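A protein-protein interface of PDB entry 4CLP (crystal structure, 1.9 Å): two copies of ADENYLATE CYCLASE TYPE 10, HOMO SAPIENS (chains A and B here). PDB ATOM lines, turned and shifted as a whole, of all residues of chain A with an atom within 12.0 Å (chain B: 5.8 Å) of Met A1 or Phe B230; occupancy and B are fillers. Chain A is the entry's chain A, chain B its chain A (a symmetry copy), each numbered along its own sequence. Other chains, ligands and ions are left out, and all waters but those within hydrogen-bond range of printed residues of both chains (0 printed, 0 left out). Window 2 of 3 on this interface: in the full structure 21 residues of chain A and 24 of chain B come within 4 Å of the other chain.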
ATOM      1  N   MET A   1     -23.519 -15.132 -10.426  1.00  0.00           N
ATOM      2  CA  MET A   1     -24.592 -15.924  -9.624  1.00  0.00           C
ATOM      3  C   MET A   1     -23.953 -16.856  -8.665  1.00  0.00           C
ATOM      4  O   MET A   1     -23.131 -17.657  -9.019  1.00  0.00           O
ATOM      5  CB  MET A   1     -25.542 -16.634 -10.577  1.00  0.00           C
ATOM      6  CG  MET A   1     -26.836 -17.253 -10.059  1.00  0.00           C
ATOM      7  SD  MET A   1     -28.311 -17.157 -11.227  1.00  0.00           S
ATOM      8  CE  MET A   1     -27.356 -17.276 -12.728  1.00  0.00           C
ATOM      9  N   ASN A   2     -24.319 -16.757  -7.398  1.00  0.00           N
ATOM     10  CA  ASN A   2     -23.721 -17.549  -6.370  1.00  0.00           C
ATOM     11  C   ASN A   2     -24.076 -19.023  -6.426  1.00  0.00           C
ATOM     12  O   ASN A   2     -25.115 -19.420  -6.950  1.00  0.00           O
ATOM     13  CB  ASN A   2     -24.121 -17.017  -4.988  1.00  0.00           C
ATOM     14  CG  ASN A   2     -23.600 -15.654  -4.711  1.00  0.00           C
ATOM     15  OD1 ASN A   2     -22.687 -15.071  -5.421  1.00  0.00           O
ATOM     16  ND2 ASN A   2     -24.265 -15.037  -3.779  1.00  0.00           N
ATOM     17  N   THR A   3     -23.186 -19.832  -5.887  1.00  0.00           N
ATOM     18  CA  THR A   3     -23.442 -21.257  -5.739  1.00  0.00           C
ATOM     19  C   THR A   3     -23.207 -21.567  -4.278  1.00  0.00           C
ATOM     20  O   THR A   3     -22.168 -22.101  -3.895  1.00  0.00           O
ATOM     21  CB  THR A   3     -22.550 -22.140  -6.685  1.00  0.00           C
ATOM     22  OG1 THR A   3     -21.204 -21.775  -6.558  1.00  0.00           O
ATOM     23  CG2 THR A   3     -22.824 -21.836  -8.087  1.00  0.00           C
ATOM     24  N   PRO A   4     -24.190 -21.235  -3.435  1.00  0.00           N
ATOM     25  CA  PRO A   4     -24.002 -21.328  -2.001  1.00  0.00           C
ATOM     26  C   PRO A   4     -23.968 -22.735  -1.473  1.00  0.00           C
ATOM     27  O   PRO A   4     -24.380 -23.653  -2.138  1.00  0.00           O
ATOM     28  CB  PRO A   4     -25.178 -20.564  -1.397  1.00  0.00           C
ATOM     29  CG  PRO A   4     -26.123 -20.307  -2.499  1.00  0.00           C
ATOM     30  CD  PRO A   4     -25.523 -20.754  -3.800  1.00  0.00           C
ATOM     31  N   LYS A   5     -23.417 -22.877  -0.269  1.00  0.00           N
ATOM     32  CA  LYS A   5     -23.304 -24.175   0.337  1.00  0.00           C
ATOM     33  C   LYS A   5     -24.708 -24.725   0.543  1.00  0.00           C
ATOM     34  O   LYS A   5     -25.636 -23.981   0.905  1.00  0.00           O
ATOM     35  CB  LYS A   5     -22.557 -24.091   1.678  1.00  0.00           C
ATOM     36  CG  LYS A   5     -22.286 -25.474   2.278  1.00  0.00           C
ATOM     37  CD  LYS A   5     -21.341 -25.438   3.468  1.00  0.00           C
ATOM     38  CE  LYS A   5     -20.802 -26.829   3.749  1.00  0.00           C
ATOM     39  NZ  LYS A   5     -19.594 -26.726   4.603  1.00  0.00           N
ATOM     40  N   ILE B  88     -30.895 -16.977  -4.892  1.00  0.00           N
ATOM     41  CA  ILE B  88     -29.688 -17.027  -5.710  1.00  0.00           C
ATOM     42  C   ILE B  88     -29.815 -16.061  -6.902  1.00  0.00           C
ATOM     43  O   ILE B  88     -28.832 -15.498  -7.307  1.00  0.00           O
ATOM     44  CB  ILE B  88     -29.465 -18.477  -6.175  1.00  0.00           C
ATOM     45  CG1 ILE B  88     -28.958 -19.320  -5.002  1.00  0.00           C
ATOM     46  CG2 ILE B  88     -28.458 -18.539  -7.319  1.00  0.00           C
ATOM     47  CD1 ILE B  88     -28.902 -20.824  -5.317  1.00  0.00           C
ATOM     48  N   PHE B  89     -31.055 -15.830  -7.382  1.00  0.00           N
ATOM     49  CA  PHE B  89     -31.369 -14.871  -8.461  1.00  0.00           C
ATOM     50  C   PHE B  89     -31.543 -13.458  -7.934  1.00  0.00           C
ATOM     51  O   PHE B  89     -31.839 -12.543  -8.717  1.00  0.00           O
ATOM     52  CB  PHE B  89     -32.591 -15.309  -9.314  1.00  0.00           C
ATOM     53  CG  PHE B  89     -32.271 -16.339 -10.364  1.00  0.00           C
ATOM     54  CD1 PHE B  89     -32.013 -17.675 -10.028  1.00  0.00           C
ATOM     55  CD2 PHE B  89     -32.179 -15.951 -11.669  1.00  0.00           C
ATOM     56  CE1 PHE B  89     -31.675 -18.612 -11.029  1.00  0.00           C
ATOM     57  CE2 PHE B  89     -31.862 -16.862 -12.698  1.00  0.00           C
ATOM     58  CZ  PHE B  89     -31.585 -18.219 -12.358  1.00  0.00           C
ATOM     59  N   GLY B  90     -31.408 -13.282  -6.605  1.00  0.00           N
ATOM     60  CA  GLY B  90     -31.308 -11.989  -6.040  1.00  0.00           C
ATOM     61  C   GLY B  90     -32.585 -11.429  -5.473  1.00  0.00           C
ATOM     62  O   GLY B  90     -32.666 -10.230  -5.113  1.00  0.00           O
ATOM     63  N   VAL B 118     -33.987 -11.210 -15.529  1.00  0.00           N
ATOM     64  CA  VAL B 118     -33.513 -11.998 -14.403  1.00  0.00           C
ATOM     65  C   VAL B 118     -34.652 -12.772 -13.743  1.00  0.00           C
ATOM     66  O   VAL B 118     -34.542 -13.984 -13.487  1.00  0.00           O
ATOM     67  CB  VAL B 118     -32.795 -11.106 -13.341  1.00  0.00           C
ATOM     68  CG1 VAL B 118     -32.469 -11.912 -12.093  1.00  0.00           C
ATOM     69  CG2 VAL B 118     -31.511 -10.458 -13.869  1.00  0.00           C
ATOM     70  N   ASN B 225     -24.581 -13.560 -22.618  1.00  0.00           N
ATOM     71  CA  ASN B 225     -24.054 -14.474 -21.622  1.00  0.00           C
ATOM     72  C   ASN B 225     -24.808 -14.214 -20.302  1.00  0.00           C
ATOM     73  O   ASN B 225     -24.670 -13.136 -19.761  1.00  0.00           O
ATOM     74  CB  ASN B 225     -22.586 -14.198 -21.412  1.00  0.00           C
ATOM     75  CG  ASN B 225     -21.987 -15.151 -20.407  1.00  0.00           C
ATOM     76  OD1 ASN B 225     -22.208 -15.041 -19.196  1.00  0.00           O
ATOM     77  ND2 ASN B 225     -21.282 -16.149 -20.913  1.00  0.00           N
ATOM     78  N   PHE B 226     -25.634 -15.147 -19.839  1.00  0.00           N
ATOM     79  CA  PHE B 226     -26.516 -14.824 -18.725  1.00  0.00           C
ATOM     80  C   PHE B 226     -25.704 -14.518 -17.477  1.00  0.00           C
ATOM     81  O   PHE B 226     -26.024 -13.614 -16.745  1.00  0.00           O
ATOM     82  CB  PHE B 226     -27.571 -15.880 -18.448  1.00  0.00           C
ATOM     83  CG  PHE B 226     -28.519 -15.439 -17.423  1.00  0.00           C
ATOM     84  CD1 PHE B 226     -29.513 -14.549 -17.743  1.00  0.00           C
ATOM     85  CD2 PHE B 226     -28.347 -15.806 -16.113  1.00  0.00           C
ATOM     86  CE1 PHE B 226     -30.376 -14.036 -16.788  1.00  0.00           C
ATOM     87  CE2 PHE B 226     -29.204 -15.312 -15.138  1.00  0.00           C
ATOM     88  CZ  PHE B 226     -30.218 -14.410 -15.482  1.00  0.00           C
ATOM     89  N   ASP B 227     -24.633 -15.254 -17.239  1.00  0.00           N
ATOM     90  CA  ASP B 227     -23.796 -14.985 -16.111  1.00  0.00           C
ATOM     91  C   ASP B 227     -23.244 -13.583 -16.093  1.00  0.00           C
ATOM     92  O   ASP B 227     -23.276 -12.900 -15.062  1.00  0.00           O
ATOM     93  CB  ASP B 227     -22.649 -15.952 -16.079  1.00  0.00           C
ATOM     94  CG  ASP B 227     -23.045 -17.255 -15.513  1.00  0.00           C
ATOM     95  OD1 ASP B 227     -24.226 -17.658 -15.662  1.00  0.00           O
ATOM     96  OD2 ASP B 227     -22.154 -17.872 -14.900  1.00  0.00           O
ATOM     97  N   GLU B 228     -22.729 -13.132 -17.214  1.00  0.00           N
ATOM     98  CA  GLU B 228     -22.195 -11.786 -17.263  1.00  0.00           C
ATOM     99  C   GLU B 228     -23.269 -10.737 -17.077  1.00  0.00           C
ATOM    100  O   GLU B 228     -23.053  -9.755 -16.402  1.00  0.00           O
ATOM    101  CB  GLU B 228     -21.421 -11.541 -18.565  1.00  0.00           C
ATOM    102  CG  GLU B 228     -20.193 -12.466 -18.587  1.00  0.00           C
ATOM    103  CD  GLU B 228     -19.320 -12.355 -19.849  1.00  0.00           C
ATOM    104  OE1 GLU B 228     -19.631 -11.544 -20.773  1.00  0.00           O
ATOM    105  OE2 GLU B 228     -18.304 -13.090 -19.845  1.00  0.00           O
ATOM    106  N   PHE B 229     -24.440 -10.966 -17.665  1.00  0.00           N
ATOM    107  CA  PHE B 229     -25.563 -10.069 -17.549  1.00  0.00           C
ATOM    108  C   PHE B 229     -26.032  -9.991 -16.074  1.00  0.00           C
ATOM    109  O   PHE B 229     -26.360  -8.922 -15.550  1.00  0.00           O
ATOM    110  CB  PHE B 229     -26.680 -10.646 -18.371  1.00  0.00           C
ATOM    111  CG  PHE B 229     -27.960  -9.905 -18.280  1.00  0.00           C
ATOM    112  CD1 PHE B 229     -28.101  -8.692 -18.852  1.00  0.00           C
ATOM    113  CD2 PHE B 229     -29.040 -10.458 -17.592  1.00  0.00           C
ATOM    114  CE1 PHE B 229     -29.308  -8.025 -18.778  1.00  0.00           C
ATOM    115  CE2 PHE B 229     -30.230  -9.803 -17.488  1.00  0.00           C
ATOM    116  CZ  PHE B 229     -30.391  -8.593 -18.088  1.00  0.00           C
ATOM    117  N   PHE B 230     -26.150 -11.159 -15.458  1.00  0.00           N
ATOM    118  CA  PHE B 230     -26.561 -11.242 -14.066  1.00  0.00           C
ATOM    119  C   PHE B 230     -25.611 -10.463 -13.248  1.00  0.00           C
ATOM    120  O   PHE B 230     -26.021  -9.692 -12.391  1.00  0.00           O
ATOM    121  CB  PHE B 230     -26.713 -12.698 -13.602  1.00  0.00           C
ATOM    122  CG  PHE B 230     -27.169 -12.827 -12.179  1.00  0.00           C
ATOM    123  CD1 PHE B 230     -28.509 -12.813 -11.870  1.00  0.00           C
ATOM    124  CD2 PHE B 230     -26.245 -12.904 -11.139  1.00  0.00           C
ATOM    125  CE1 PHE B 230     -28.911 -12.893 -10.577  1.00  0.00           C
ATOM    126  CE2 PHE B 230     -26.632 -12.937  -9.843  1.00  0.00           C
ATOM    127  CZ  PHE B 230     -27.973 -12.948  -9.555  1.00  0.00           C
ATOM    128  N   THR B 231     -24.313 -10.604 -13.527  1.00  0.00           N
ATOM    129  CA  THR B 231     -23.338  -9.897 -12.745  1.00  0.00           C
ATOM    130  C   THR B 231     -23.566  -8.381 -12.840  1.00  0.00           C
ATOM    131  O   THR B 231     -23.512  -7.714 -11.834  1.00  0.00           O
ATOM    132  CB  THR B 231     -21.921 -10.314 -13.122  1.00  0.00           C
ATOM    133  OG1 THR B 231     -21.749 -11.673 -12.753  1.00  0.00           O
ATOM    134  CG2 THR B 231     -20.883  -9.481 -12.379  1.00  0.00           C
ATOM    135  N   LYS B 232     -23.829  -7.851 -14.034  1.00  0.00           N
ATOM    136  CA  LYS B 232     -24.145  -6.458 -14.194  1.00  0.00           C
ATOM    137  C   LYS B 232     -25.325  -6.063 -13.361  1.00  0.00           C
ATOM    138  O   LYS B 232     -25.244  -5.071 -12.677  1.00  0.00           O
ATOM    139  CB  LYS B 232     -24.401  -6.037 -15.654  1.00  0.00           C
ATOM    140  CG  LYS B 232     -23.161  -6.136 -16.522  1.00  0.00           C
ATOM    141  CD  LYS B 232     -23.520  -6.007 -18.016  1.00  0.00           C
ATOM    142  CE  LYS B 232     -22.297  -5.822 -18.914  1.00  0.00           C
ATOM    143  NZ  LYS B 232     -22.695  -5.047 -20.130  1.00  0.00           N
ATOM    144  N   CYS B 233     -26.403  -6.834 -13.410  1.00  0.00           N
ATOM    145  CA  CYS B 233     -27.584  -6.560 -12.598  1.00  0.00           C
ATOM    146  C   CYS B 233     -27.315  -6.506 -11.058  1.00  0.00           C
ATOM    147  O   CYS B 233     -28.036  -5.798 -10.340  1.00  0.00           O
ATOM    148  CB  CYS B 233     -28.663  -7.606 -12.898  1.00  0.00           C
ATOM    149  SG  CYS B 233     -29.324  -7.521 -14.567  1.00  0.00           S
ATOM    150  N   THR B 234     -26.324  -7.293 -10.585  1.00  0.00           N
ATOM    151  CA  THR B 234     -25.998  -7.390  -9.135  1.00  0.00           C
ATOM    152  C   THR B 234     -25.439  -6.041  -8.634  1.00  0.00           C
ATOM    153  O   THR B 234     -25.552  -5.745  -7.460  1.00  0.00           O
ATOM    154  CB  THR B 234     -25.024  -8.515  -8.733  1.00  0.00           C
ATOM    155  OG1 THR B 234     -23.759  -8.351  -9.369  1.00  0.00           O
ATOM    156  CG2 THR B 234     -25.536  -9.837  -9.066  1.00  0.00           C
ATOM    157  N   THR B 235     -24.945  -5.190  -9.530  1.00  0.00           N
ATOM    158  CA  THR B 235     -24.548  -3.818  -9.125  1.00  0.00           C
ATOM    159  C   THR B 235     -25.660  -3.066  -8.467  1.00  0.00           C
ATOM    160  O   THR B 235     -25.464  -2.203  -7.586  1.00  0.00           O
ATOM    161  CB  THR B 235     -24.296  -3.039 -10.386  1.00  0.00           C
ATOM    162  OG1 THR B 235     -23.099  -3.502 -10.864  1.00  0.00           O
ATOM    163  CG2 THR B 235     -24.190  -1.591 -10.156  1.00  0.00           C
ATOM    164  N   MET B 237     -28.171  -4.528  -6.807  1.00  0.00           N
ATOM    165  CA  MET B 237     -28.810  -5.322  -5.745  1.00  0.00           C
ATOM    166  C   MET B 237     -28.056  -5.107  -4.413  1.00  0.00           C
ATOM    167  O   MET B 237     -26.933  -5.619  -4.218  1.00  0.00           O
ATOM    168  CB  MET B 237     -28.775  -6.825  -6.070  1.00  0.00           C
ATOM    169  CG  MET B 237     -29.591  -7.268  -7.304  1.00  0.00           C
ATOM    170  SD  MET B 237     -29.221  -9.024  -7.708  1.00  0.00           S
ATOM    171  CE  MET B 237     -30.130  -9.111  -9.260  1.00  0.00           C
ATOM    172  N   TYR B 240     -27.099  -8.500  -2.158  1.00  0.00           N
ATOM    173  CA  TYR B 240     -26.684  -9.733  -2.772  1.00  0.00           C
ATOM    174  C   TYR B 240     -25.382 -10.262  -2.093  1.00  0.00           C
ATOM    175  O   TYR B 240     -24.388  -9.570  -2.035  1.00  0.00           O
ATOM    176  CB  TYR B 240     -26.499  -9.595  -4.300  1.00  0.00           C
ATOM    177  CG  TYR B 240     -26.447 -10.970  -4.989  1.00  0.00           C
ATOM    178  CD1 TYR B 240     -27.562 -11.769  -5.033  1.00  0.00           C
ATOM    179  CD2 TYR B 240     -25.320 -11.441  -5.603  1.00  0.00           C
ATOM    180  CE1 TYR B 240     -27.535 -13.025  -5.632  1.00  0.00           C
ATOM    181  CE2 TYR B 240     -25.283 -12.693  -6.206  1.00  0.00           C
ATOM    182  CZ  TYR B 240     -26.409 -13.476  -6.248  1.00  0.00           C
ATOM    183  OH  TYR B 240     -26.433 -14.746  -6.830  1.00  0.00           O
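Printed residues of chain A that touch a printed residue of chain B: Met A1, Asn A2 and Pro A4. Hydrophobic or aromatic side chains of chain A within 4 Å of the printed part of chain B: Met A1 and Pro A4. Of the 17 printed residues of chain B, 5 touch a printed residue of chain A. Along chain B the printed residues that touch a printed residue of chain A span positions 88 to 240.
No position is printed for both chains.
Met A1 touches just these residues of chain B: Ile B88, Phe B89, Phe B226, Phe B230 and Tyr B240. Printed residues of chain B within 4 Å of Asn A2: Ile B88 (3.5 Å) and Tyr B240 (3.0 Å). Printed residues of chain B within 4 Å of Pro A4: Ile B88 (3.7 Å). Of chain A, only Met A1 (3.6 Å) comes within 4 Å of Phe B89. No residue of chain A comes within 4 Å of Val B118. No residue of chain A comes within 4 Å of Phe B229. Phe B230 touches just one residue of chain A: Met A1 (3.6 Å). No residue of chain A comes within 4 Å of Thr B231. Lys B232 touches none of the printed residues of chain A. No residue of chain A comes within 4 Å of Cys B233. Of the printed residues of chain A, Tyr B240 touches Met A1 and Asn A2. The nearest printed residue of chain B that does not touch Pro A4 is Tyr B240 (6.8 Å).
OH of Tyr B240 is in hydrogen-bond range of O of Ile B88.
Met A1 touches Ile B88 (CG to CG2, 3.4 Å). Phe B89 touches Met A1. CE of Met A1 touches CE2 of Phe B226, at 3.6 Å. Met A1 touches Phe B230 (N to CD2, 3.6 Å). Met A1 touches Tyr B240. Asn A2 touches Ile B88. Pro A4 touches Ile B88.
N of Asn A2 is in hydrogen-bond range of OH of Tyr B240, 3.0 Å away.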
